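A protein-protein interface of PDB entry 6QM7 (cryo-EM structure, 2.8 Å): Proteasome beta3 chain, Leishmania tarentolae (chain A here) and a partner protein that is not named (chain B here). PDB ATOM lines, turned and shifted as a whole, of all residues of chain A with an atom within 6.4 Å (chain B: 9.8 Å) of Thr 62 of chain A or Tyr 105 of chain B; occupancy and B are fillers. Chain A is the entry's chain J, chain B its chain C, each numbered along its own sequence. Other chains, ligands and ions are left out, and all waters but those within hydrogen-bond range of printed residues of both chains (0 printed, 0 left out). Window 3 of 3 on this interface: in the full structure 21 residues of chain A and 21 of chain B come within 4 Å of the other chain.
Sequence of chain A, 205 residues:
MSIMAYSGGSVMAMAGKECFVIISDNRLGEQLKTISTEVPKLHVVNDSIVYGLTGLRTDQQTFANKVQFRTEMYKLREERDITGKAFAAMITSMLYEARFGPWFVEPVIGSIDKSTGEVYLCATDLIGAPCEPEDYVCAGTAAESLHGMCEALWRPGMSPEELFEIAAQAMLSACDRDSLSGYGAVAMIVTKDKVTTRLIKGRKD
Among the printed residues, pairs that only touch across the chains: Asn 65 of chain A with Tyr 105 of chain B, Thr 62 of chain A with Tyr 105 of chain B, Lys 66 of chain A with Tyr 105 of chain B, Phe 69 of chain A with Leu 101 of chain B, Phe 69 of chain A with Leu 98 of chain B and Phe 69 of chain A with Arg 102 of chain B.
The backbone carbonyl oxygen of Thr 58 of chain A is in hydrogen-bond range of the side-chain hydroxyl of Thr 62 of chain A (3.1 Å). The backbone carbonyl oxygen (O) of Gln 61 of chain A sits close to the side-chain amide nitrogen (ND2) of Asn 65 of chain A (3.3 Å). O of Arg 102 of chain B sits at hydrogen-bond distance from OG1 of Thr 106 of chain B. The backbone carbonyl oxygen (O) of Gln 104 of chain B is in hydrogen-bond range of the side-chain amide nitrogen (NE2) of Gln 108 of chain B (3.0 Å). The backbone carbonyl oxygen (O) of Tyr 105 of chain B lies within hydrogen-bond range of the side-chain amide nitrogen (NE2) of Gln 108 of chain B (2.7 Å).
The side-chain amide nitrogen of Asn 65 of chain A sits close to the side-chain amide nitrogen of Gln 108 of chain B. The side-chain amide oxygen of Gln 104 of chain B sits at hydrogen-bond distance from the side-chain amide nitrogen of Gln 68 of chain A (3.2 Å). OE1 of Gln 68 of chain A sits close to OE1 of Gln 108 of chain B, at 3.3 Å.
Printed residues of chain B that touch a printed residue of chain A: Leu 98, Leu 101, Arg 102, Gln 104, Tyr 105 and Gln 108. Of the 14 printed residues of chain A, 5 touch a printed residue of chain B. Printed residues of chain A that touch a printed residue of chain B: Thr 62, Asn 65, Lys 66, Gln 68 and Phe 69. Among the printed residues, 9 pairs touch across the chains. Among the printed residues, no Asp or Glu carboxylate lies within 4 Å of a Lys or Arg side-chain nitrogen of the other chain.
Thr 62 of chain A touches just one residue of chain B: Tyr 105. Of the printed residues of chain B, Gln 68 of chain A touches Gln 104 and Gln 108. Of the printed residues of chain B, Phe 69 of chain A touches Leu 98, Leu 101 and Arg 102. Of the printed residues of chain A, Leu 98 of chain B touches Phe 69 (3.8 Å). Printed residues of chain A within 4 Å of Arg 102 of chain B: Phe 69. Tyr 105 of chain B touches three residues of chain A. The nearest residue of chain B that does not touch Thr 62 of chain A is Gln 108 of chain B (7.1 Å). The nearest residue of chain A that does not touch Tyr 105 of chain B is Phe 69 of chain A (4.4 Å). The nearest printed residue of chain A that does not touch Arg 102 of chain B is Asn 65 of chain A (8.5 Å).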
ATOM      1  N   ARG A  57      -7.151  18.068  -8.256  1.00  0.00           N
ATOM      2  CA  ARG A  57      -8.411  17.339  -7.946  1.00  0.00           C
ATOM      3  C   ARG A  57      -8.483  17.003  -6.458  1.00  0.00           C
ATOM      4  O   ARG A  57      -9.573  17.146  -5.891  1.00  0.00           O
ATOM      5  CB  ARG A  57      -8.553  16.035  -8.736  1.00  0.00           C
ATOM      6  CG  ARG A  57      -9.819  15.245  -8.443  1.00  0.00           C
ATOM      7  CD  ARG A  57     -11.044  16.088  -8.693  1.00  0.00           C
ATOM      8  NE  ARG A  57     -12.249  15.377  -8.323  1.00  0.00           N
ATOM      9  CZ  ARG A  57     -13.448  15.930  -8.242  1.00  0.00           C
ATOM     10  NH1 ARG A  57     -13.626  17.214  -8.500  1.00  0.00           N
ATOM     11  NH2 ARG A  57     -14.478  15.188  -7.895  1.00  0.00           N
ATOM     12  N   THR A  58      -7.377  16.529  -5.881  1.00  0.00           N
ATOM     13  CA  THR A  58      -7.202  16.367  -4.418  1.00  0.00           C
ATOM     14  C   THR A  58      -7.785  17.556  -3.659  1.00  0.00           C
ATOM     15  O   THR A  58      -8.509  17.337  -2.703  1.00  0.00           O
ATOM     16  CB  THR A  58      -5.742  16.434  -3.971  1.00  0.00           C
ATOM     17  OG1 THR A  58      -4.864  16.069  -5.030  1.00  0.00           O
ATOM     18  CG2 THR A  58      -5.542  15.576  -2.749  1.00  0.00           C
ATOM     19  N   ASP A  59      -7.406  18.769  -4.056  1.00  0.00           N
ATOM     20  CA  ASP A  59      -7.740  20.002  -3.312  1.00  0.00           C
ATOM     21  C   ASP A  59      -9.189  20.361  -3.610  1.00  0.00           C
ATOM     22  O   ASP A  59      -9.869  20.794  -2.689  1.00  0.00           O
ATOM     23  CB  ASP A  59      -6.758  21.129  -3.623  1.00  0.00           C
ATOM     24  CG  ASP A  59      -5.375  20.913  -3.034  1.00  0.00           C
ATOM     25  OD1 ASP A  59      -4.566  21.862  -3.071  1.00  0.00           O
ATOM     26  OD2 ASP A  59      -5.114  19.795  -2.521  1.00  0.00           O
ATOM     27  N   GLN A  60      -9.653  20.162  -4.833  1.00  0.00           N
ATOM     28  CA  GLN A  60     -11.094  20.299  -5.123  1.00  0.00           C
ATOM     29  C   GLN A  60     -11.854  19.412  -4.141  1.00  0.00           C
ATOM     30  O   GLN A  60     -12.847  19.878  -3.601  1.00  0.00           O
ATOM     31  CB  GLN A  60     -11.490  19.845  -6.524  1.00  0.00           C
ATOM     32  CG  GLN A  60     -10.687  20.464  -7.646  1.00  0.00           C
ATOM     33  CD  GLN A  60     -11.182  19.957  -8.966  1.00  0.00           C
ATOM     34  OE1 GLN A  60     -12.325  19.529  -9.090  1.00  0.00           O
ATOM     35  NE2 GLN A  60     -10.316  20.015  -9.960  1.00  0.00           N
ATOM     36  N   GLN A  61     -11.404  18.180  -3.921  1.00  0.00           N
ATOM     37  CA  GLN A  61     -12.145  17.207  -3.081  1.00  0.00           C
ATOM     38  C   GLN A  61     -11.998  17.561  -1.607  1.00  0.00           C
ATOM     39  O   GLN A  61     -13.016  17.489  -0.907  1.00  0.00           O
ATOM     40  CB  GLN A  61     -11.685  15.780  -3.336  1.00  0.00           C
ATOM     41  CG  GLN A  61     -12.109  15.300  -4.707  1.00  0.00           C
ATOM     42  CD  GLN A  61     -11.824  13.837  -4.885  1.00  0.00           C
ATOM     43  OE1 GLN A  61     -10.669  13.419  -4.929  1.00  0.00           O
ATOM     44  NE2 GLN A  61     -12.885  13.057  -5.004  1.00  0.00           N
ATOM     45  N   THR A  62     -10.789  17.892  -1.162  1.00  0.00           N
ATOM     46  CA  THR A  62     -10.523  18.282   0.242  1.00  0.00           C
ATOM     47  C   THR A  62     -11.256  19.588   0.513  1.00  0.00           C
ATOM     48  O   THR A  62     -12.049  19.622   1.449  1.00  0.00           O
ATOM     49  CB  THR A  62      -9.042  18.456   0.588  1.00  0.00           C
ATOM     50  OG1 THR A  62      -8.300  17.260   0.361  1.00  0.00           O
ATOM     51  CG2 THR A  62      -8.845  18.803   2.046  1.00  0.00           C
ATOM     52  N   PHE A  63     -11.010  20.613  -0.286  1.00  0.00           N
ATOM     53  CA  PHE A  63     -11.651  21.939  -0.114  1.00  0.00           C
ATOM     54  C   PHE A  63     -13.171  21.786  -0.131  1.00  0.00           C
ATOM     55  O   PHE A  63     -13.802  22.368   0.740  1.00  0.00           O
ATOM     56  CB  PHE A  63     -11.211  22.936  -1.182  1.00  0.00           C
ATOM     57  CG  PHE A  63     -11.583  24.341  -0.822  1.00  0.00           C
ATOM     58  CD1 PHE A  63     -10.878  25.018   0.163  1.00  0.00           C
ATOM     59  CD2 PHE A  63     -12.682  24.949  -1.400  1.00  0.00           C
ATOM     60  CE1 PHE A  63     -11.231  26.309   0.522  1.00  0.00           C
ATOM     61  CE2 PHE A  63     -13.032  26.241  -1.044  1.00  0.00           C
ATOM     62  CZ  PHE A  63     -12.310  26.914  -0.081  1.00  0.00           C
ATOM     63  N   ALA A  64     -13.732  21.029  -1.073  1.00  0.00           N
ATOM     64  CA  ALA A  64     -15.194  20.825  -1.187  1.00  0.00           C
ATOM     65  C   ALA A  64     -15.728  20.206   0.104  1.00  0.00           C
ATOM     66  O   ALA A  64     -16.848  20.588   0.510  1.00  0.00           O
ATOM     67  CB  ALA A  64     -15.558  19.955  -2.362  1.00  0.00           C
ATOM     68  N   ASN A  65     -14.989  19.264   0.693  1.00  0.00           N
ATOM     69  CA  ASN A  65     -15.374  18.617   1.969  1.00  0.00           C
ATOM     70  C   ASN A  65     -15.376  19.667   3.069  1.00  0.00           C
ATOM     71  O   ASN A  65     -16.305  19.656   3.875  1.00  0.00           O
ATOM     72  CB  ASN A  65     -14.406  17.526   2.430  1.00  0.00           C
ATOM     73  CG  ASN A  65     -14.501  16.214   1.690  1.00  0.00           C
ATOM     74  OD1 ASN A  65     -13.719  15.307   1.976  1.00  0.00           O
ATOM     75  ND2 ASN A  65     -15.441  16.107   0.763  1.00  0.00           N
ATOM     76  N   LYS A  66     -14.299  20.448   3.154  1.00  0.00           N
ATOM     77  CA  LYS A  66     -14.113  21.498   4.181  1.00  0.00           C
ATOM     78  C   LYS A  66     -15.270  22.474   4.090  1.00  0.00           C
ATOM     79  O   LYS A  66     -15.741  22.882   5.127  1.00  0.00           O
ATOM     80  CB  LYS A  66     -12.842  22.310   3.961  1.00  0.00           C
ATOM     81  CG  LYS A  66     -11.552  21.667   4.436  1.00  0.00           C
ATOM     82  CD  LYS A  66     -10.422  22.684   4.541  1.00  0.00           C
ATOM     83  CE  LYS A  66      -9.643  22.555   5.831  1.00  0.00           C
ATOM     84  NZ  LYS A  66      -9.205  21.151   6.067  1.00  0.00           N
ATOM     85  N   VAL A  67     -15.678  22.828   2.878  1.00  0.00           N
ATOM     86  CA  VAL A  67     -16.800  23.772   2.632  1.00  0.00           C
ATOM     87  C   VAL A  67     -18.097  23.102   3.068  1.00  0.00           C
ATOM     88  O   VAL A  67     -18.913  23.794   3.671  1.00  0.00           O
ATOM     89  CB  VAL A  67     -16.860  24.210   1.157  1.00  0.00           C
ATOM     90  CG1 VAL A  67     -18.197  24.843   0.796  1.00  0.00           C
ATOM     91  CG2 VAL A  67     -15.712  25.149   0.826  1.00  0.00           C
ATOM     92  N   GLN A  68     -18.288  21.833   2.723  1.00  0.00           N
ATOM     93  CA  GLN A  68     -19.520  21.081   3.057  1.00  0.00           C
ATOM     94  C   GLN A  68     -19.655  20.993   4.578  1.00  0.00           C
ATOM     95  O   GLN A  68     -20.785  21.031   5.067  1.00  0.00           O
ATOM     96  CB  GLN A  68     -19.490  19.693   2.425  1.00  0.00           C
ATOM     97  CG  GLN A  68     -20.809  18.932   2.493  1.00  0.00           C
ATOM     98  CD  GLN A  68     -20.555  17.444   2.462  1.00  0.00           C
ATOM     99  OE1 GLN A  68     -20.069  16.902   1.468  1.00  0.00           O
ATOM    100  NE2 GLN A  68     -20.847  16.774   3.568  1.00  0.00           N
ATOM    101  N   PHE A  69     -18.542  20.894   5.297  1.00  0.00           N
ATOM    102  CA  PHE A  69     -18.489  20.933   6.780  1.00  0.00           C
ATOM    103  C   PHE A  69     -18.978  22.308   7.246  1.00  0.00           C
ATOM    104  O   PHE A  69     -19.889  22.394   8.077  1.00  0.00           O
ATOM    105  CB  PHE A  69     -17.070  20.608   7.247  1.00  0.00           C
ATOM    106  CG  PHE A  69     -16.839  20.730   8.728  1.00  0.00           C
ATOM    107  CD1 PHE A  69     -16.881  19.619   9.540  1.00  0.00           C
ATOM    108  CD2 PHE A  69     -16.547  21.960   9.298  1.00  0.00           C
ATOM    109  CE1 PHE A  69     -16.670  19.738  10.902  1.00  0.00           C
ATOM    110  CE2 PHE A  69     -16.339  22.080  10.659  1.00  0.00           C
ATOM    111  CZ  PHE A  69     -16.411  20.969  11.457  1.00  0.00           C
ATOM    112  N   TRP A 103      -4.451  26.118  -1.026  1.00  0.00           N
ATOM    113  CA  TRP A 103      -5.269  25.104  -1.727  1.00  0.00           C
ATOM    114  C   TRP A 103      -5.165  25.412  -3.207  1.00  0.00           C
ATOM    115  O   TRP A 103      -5.476  26.538  -3.563  1.00  0.00           O
ATOM    116  CB  TRP A 103      -6.737  25.161  -1.295  1.00  0.00           C
ATOM    117  CG  TRP A 103      -6.939  24.921   0.163  1.00  0.00           C
ATOM    118  CD1 TRP A 103      -7.262  25.834   1.118  1.00  0.00           C
ATOM    119  CD2 TRP A 103      -6.793  23.666   0.834  1.00  0.00           C
ATOM    120  NE1 TRP A 103      -7.331  25.231   2.342  1.00  0.00           N
ATOM    121  CE2 TRP A 103      -7.050  23.901   2.199  1.00  0.00           C
ATOM    122  CE3 TRP A 103      -6.470  22.370   0.407  1.00  0.00           C
ATOM    123  CZ2 TRP A 103      -6.987  22.885   3.148  1.00  0.00           C
ATOM    124  CZ3 TRP A 103      -6.412  21.363   1.340  1.00  0.00           C
ATOM    125  CH2 TRP A 103      -6.671  21.620   2.692  1.00  0.00           C
ATOM    126  N   ARG B  97     -22.622  18.292  17.293  1.00  0.00           N
ATOM    127  CA  ARG B  97     -22.834  18.762  15.903  1.00  0.00           C
ATOM    128  C   ARG B  97     -21.480  18.692  15.187  1.00  0.00           C
ATOM    129  O   ARG B  97     -21.432  18.157  14.077  1.00  0.00           O
ATOM    130  CB  ARG B  97     -23.441  20.170  15.856  1.00  0.00           C
ATOM    131  CG  ARG B  97     -24.618  20.367  16.802  1.00  0.00           C
ATOM    132  CD  ARG B  97     -25.929  20.891  16.248  1.00  0.00           C
ATOM    133  NE  ARG B  97     -26.158  22.289  16.544  1.00  0.00           N
ATOM    134  CZ  ARG B  97     -27.348  22.864  16.665  1.00  0.00           C
ATOM    135  NH1 ARG B  97     -28.480  22.189  16.531  1.00  0.00           N
ATOM    136  NH2 ARG B  97     -27.408  24.156  16.919  1.00  0.00           N
ATOM    137  N   LEU B  98     -20.423  19.188  15.826  1.00  0.00           N
ATOM    138  CA  LEU B  98     -19.054  19.160  15.267  1.00  0.00           C
ATOM    139  C   LEU B  98     -18.617  17.715  15.060  1.00  0.00           C
ATOM    140  O   LEU B  98     -18.045  17.438  13.996  1.00  0.00           O
ATOM    141  CB  LEU B  98     -18.073  19.885  16.193  1.00  0.00           C
ATOM    142  CG  LEU B  98     -18.125  21.413  16.162  1.00  0.00           C
ATOM    143  CD1 LEU B  98     -17.020  22.006  17.029  1.00  0.00           C
ATOM    144  CD2 LEU B  98     -18.012  21.952  14.737  1.00  0.00           C
ATOM    145  N   SER B  99     -18.844  16.844  16.033  1.00  0.00           N
ATOM    146  CA  SER B  99     -18.387  15.436  15.971  1.00  0.00           C
ATOM    147  C   SER B  99     -19.082  14.717  14.818  1.00  0.00           C
ATOM    148  O   SER B  99     -18.386  14.009  14.073  1.00  0.00           O
ATOM    149  CB  SER B  99     -18.604  14.727  17.265  1.00  0.00           C
ATOM    150  OG  SER B  99     -17.710  15.222  18.256  1.00  0.00           O
ATOM    151  N   ALA B 100     -20.392  14.904  14.676  1.00  0.00           N
ATOM    152  CA  ALA B 100     -21.201  14.307  13.594  1.00  0.00           C
ATOM    153  C   ALA B 100     -20.663  14.778  12.244  1.00  0.00           C
ATOM    154  O   ALA B 100     -20.575  13.949  11.326  1.00  0.00           O
ATOM    155  CB  ALA B 100     -22.659  14.646  13.750  1.00  0.00           C
ATOM    156  N   LEU B 101     -20.301  16.053  12.130  1.00  0.00           N
ATOM    157  CA  LEU B 101     -19.801  16.633  10.863  1.00  0.00           C
ATOM    158  C   LEU B 101     -18.343  16.249  10.643  1.00  0.00           C
ATOM    159  O   LEU B 101     -17.975  16.122   9.462  1.00  0.00           O
ATOM    160  CB  LEU B 101     -19.971  18.152  10.873  1.00  0.00           C
ATOM    161  CG  LEU B 101     -21.413  18.659  10.831  1.00  0.00           C
ATOM    162  CD1 LEU B 101     -21.442  20.127  10.442  1.00  0.00           C
ATOM    163  CD2 LEU B 101     -22.301  17.845   9.887  1.00  0.00           C
ATOM    164  N   ARG B 102     -17.542  16.118  11.705  1.00  0.00           N
ATOM    165  CA  ARG B 102     -16.121  15.693  11.581  1.00  0.00           C
ATOM    166  C   ARG B 102     -16.120  14.267  11.049  1.00  0.00           C
ATOM    167  O   ARG B 102     -15.258  13.970  10.208  1.00  0.00           O
ATOM    168  CB  ARG B 102     -15.318  15.820  12.880  1.00  0.00           C
ATOM    169  CG  ARG B 102     -14.660  17.184  13.051  1.00  0.00           C
ATOM    170  CD  ARG B 102     -13.668  17.289  14.200  1.00  0.00           C
ATOM    171  NE  ARG B 102     -14.011  18.364  15.130  1.00  0.00           N
ATOM    172  CZ  ARG B 102     -14.639  18.224  16.311  1.00  0.00           C
ATOM    173  NH1 ARG B 102     -15.020  17.036  16.759  1.00  0.00           N
ATOM    174  NH2 ARG B 102     -14.882  19.296  17.050  1.00  0.00           N
ATOM    175  N   HIS B 103     -17.068  13.433  11.481  1.00  0.00           N
ATOM    176  CA  HIS B 103     -17.233  12.056  10.940  1.00  0.00           C
ATOM    177  C   HIS B 103     -17.603  12.140   9.461  1.00  0.00           C
ATOM    178  O   HIS B 103     -16.968  11.480   8.661  1.00  0.00           O
ATOM    179  CB  HIS B 103     -18.260  11.251  11.732  1.00  0.00           C
ATOM    180  CG  HIS B 103     -18.382   9.850  11.249  1.00  0.00           C
ATOM    181  ND1 HIS B 103     -17.743   8.796  11.873  1.00  0.00           N
ATOM    182  CD2 HIS B 103     -19.054   9.327  10.205  1.00  0.00           C
ATOM    183  CE1 HIS B 103     -18.027   7.678  11.231  1.00  0.00           C
ATOM    184  NE2 HIS B 103     -18.823   7.979  10.194  1.00  0.00           N
ATOM    185  N   GLN B 104     -18.604  12.939   9.122  1.00  0.00           N
ATOM    186  CA  GLN B 104     -19.047  13.113   7.723  1.00  0.00           C
ATOM    187  C   GLN B 104     -17.899  13.672   6.885  1.00  0.00           C
ATOM    188  O   GLN B 104     -17.830  13.345   5.707  1.00  0.00           O
ATOM    189  CB  GLN B 104     -20.252  14.041   7.660  1.00  0.00           C
ATOM    190  CG  GLN B 104     -20.721  14.324   6.238  1.00  0.00           C
ATOM    191  CD  GLN B 104     -22.167  14.746   6.258  1.00  0.00           C
ATOM    192  OE1 GLN B 104     -22.484  15.942   6.237  1.00  0.00           O
ATOM    193  NE2 GLN B 104     -23.041  13.754   6.365  1.00  0.00           N
ATOM    194  N   TYR B 105     -17.058  14.534   7.450  1.00  0.00           N
ATOM    195  CA  TYR B 105     -15.878  15.073   6.738  1.00  0.00           C
ATOM    196  C   TYR B 105     -15.013  13.887   6.342  1.00  0.00           C
ATOM    197  O   TYR B 105     -14.733  13.723   5.143  1.00  0.00           O
ATOM    198  CB  TYR B 105     -15.080  16.061   7.589  1.00  0.00           C
ATOM    199  CG  TYR B 105     -13.832  16.562   6.917  1.00  0.00           C
ATOM    200  CD1 TYR B 105     -13.875  17.614   6.022  1.00  0.00           C
ATOM    201  CD2 TYR B 105     -12.612  15.961   7.150  1.00  0.00           C
ATOM    202  CE1 TYR B 105     -12.731  18.070   5.387  1.00  0.00           C
ATOM    203  CE2 TYR B 105     -11.457  16.407   6.528  1.00  0.00           C
ATOM    204  CZ  TYR B 105     -11.513  17.465   5.639  1.00  0.00           C
ATOM    205  OH  TYR B 105     -10.372  17.893   5.025  1.00  0.00           O
ATOM    206  N   THR B 106     -14.643  13.070   7.326  1.00  0.00           N
ATOM    207  CA  THR B 106     -13.656  11.981   7.146  1.00  0.00           C
ATOM    208  C   THR B 106     -14.236  10.902   6.233  1.00  0.00           C
ATOM    209  O   THR B 106     -13.622  10.645   5.205  1.00  0.00           O
ATOM    210  CB  THR B 106     -13.181  11.412   8.479  1.00  0.00           C
ATOM    211  OG1 THR B 106     -12.627  12.473   9.257  1.00  0.00           O
ATOM    212  CG2 THR B 106     -12.143  10.338   8.268  1.00  0.00           C
ATOM    213  N   PHE B 107     -15.403  10.367   6.550  1.00  0.00           N
ATOM    214  CA  PHE B 107     -15.962   9.155   5.919  1.00  0.00           C
ATOM    215  C   PHE B 107     -16.978   9.485   4.826  1.00  0.00           C
ATOM    216  O   PHE B 107     -17.325   8.559   4.075  1.00  0.00           O
ATOM    217  CB  PHE B 107     -16.552   8.265   7.007  1.00  0.00           C
ATOM    218  CG  PHE B 107     -15.515   7.852   8.016  1.00  0.00           C
ATOM    219  CD1 PHE B 107     -14.647   6.806   7.751  1.00  0.00           C
ATOM    220  CD2 PHE B 107     -15.349   8.555   9.193  1.00  0.00           C
ATOM    221  CE1 PHE B 107     -13.653   6.452   8.647  1.00  0.00           C
ATOM    222  CE2 PHE B 107     -14.353   8.208  10.088  1.00  0.00           C
ATOM    223  CZ  PHE B 107     -13.506   7.159   9.813  1.00  0.00           C
ATOM    224  N   GLN B 108     -17.430  10.732   4.695  1.00  0.00           N
ATOM    225  CA  GLN B 108     -18.444  11.147   3.681  1.00  0.00           C
ATOM    226  C   GLN B 108     -19.653  10.219   3.776  1.00  0.00           C
ATOM    227  O   GLN B 108     -20.211   9.860   2.732  1.00  0.00           O
ATOM    228  CB  GLN B 108     -17.842  11.196   2.273  1.00  0.00           C
ATOM    229  CG  GLN B 108     -16.781  12.284   2.108  1.00  0.00           C
ATOM    230  CD  GLN B 108     -17.293  13.668   2.447  1.00  0.00           C
ATOM    231  OE1 GLN B 108     -18.373  14.075   2.012  1.00  0.00           O
ATOM    232  NE2 GLN B 108     -16.527  14.403   3.239  1.00  0.00           N
ATOM    233  N   GLU B 109     -20.031   9.866   5.002  1.00  0.00           N
ATOM    234  CA  GLU B 109     -21.270   9.123   5.311  1.00  0.00           C
ATOM    235  C   GLU B 109     -21.785   9.620   6.652  1.00  0.00           C
ATOM    236  O   GLU B 109     -21.021  10.148   7.443  1.00  0.00           O
ATOM    237  CB  GLU B 109     -21.019   7.613   5.327  1.00  0.00           C
ATOM    238  CG  GLU B 109     -19.985   7.168   6.349  1.00  0.00           C
ATOM    239  CD  GLU B 109     -20.223   5.814   7.010  1.00  0.00           C
ATOM    240  OE1 GLU B 109     -19.724   5.622   8.153  1.00  0.00           O
ATOM    241  OE2 GLU B 109     -20.888   4.944   6.387  1.00  0.00           O
ATOM    242  N   PRO B 110     -23.095   9.507   6.941  1.00  0.00           N
ATOM    243  CA  PRO B 110     -23.616   9.887   8.249  1.00  0.00           C
ATOM    244  C   PRO B 110     -23.060   8.996   9.364  1.00  0.00           C
ATOM    245  O   PRO B 110     -22.984   7.798   9.190  1.00  0.00           O
ATOM    246  CB  PRO B 110     -25.129   9.703   8.120  1.00  0.00           C
ATOM    247  CG  PRO B 110     -25.267   8.708   6.993  1.00  0.00           C
ATOM    248  CD  PRO B 110     -24.153   9.055   6.031  1.00  0.00           C
ATOM    249  N   MET B 111     -22.655   9.638  10.456  1.00  0.00           N
ATOM    250  CA  MET B 111     -22.197   8.985  11.701  1.00  0.00           C
ATOM    251  C   MET B 111     -23.308   8.090  12.231  1.00  0.00           C
ATOM    252  O   MET B 111     -24.468   8.547  12.288  1.00  0.00           O
ATOM    253  CB  MET B 111     -21.883  10.033  12.769  1.00  0.00           C
ATOM    254  CG  MET B 111     -21.015   9.497  13.857  1.00  0.00           C
ATOM    255  SD  MET B 111     -20.462  10.816  14.910  1.00  0.00           S
ATOM    256  CE  MET B 111     -18.903  10.137  15.482  1.00  0.00           C
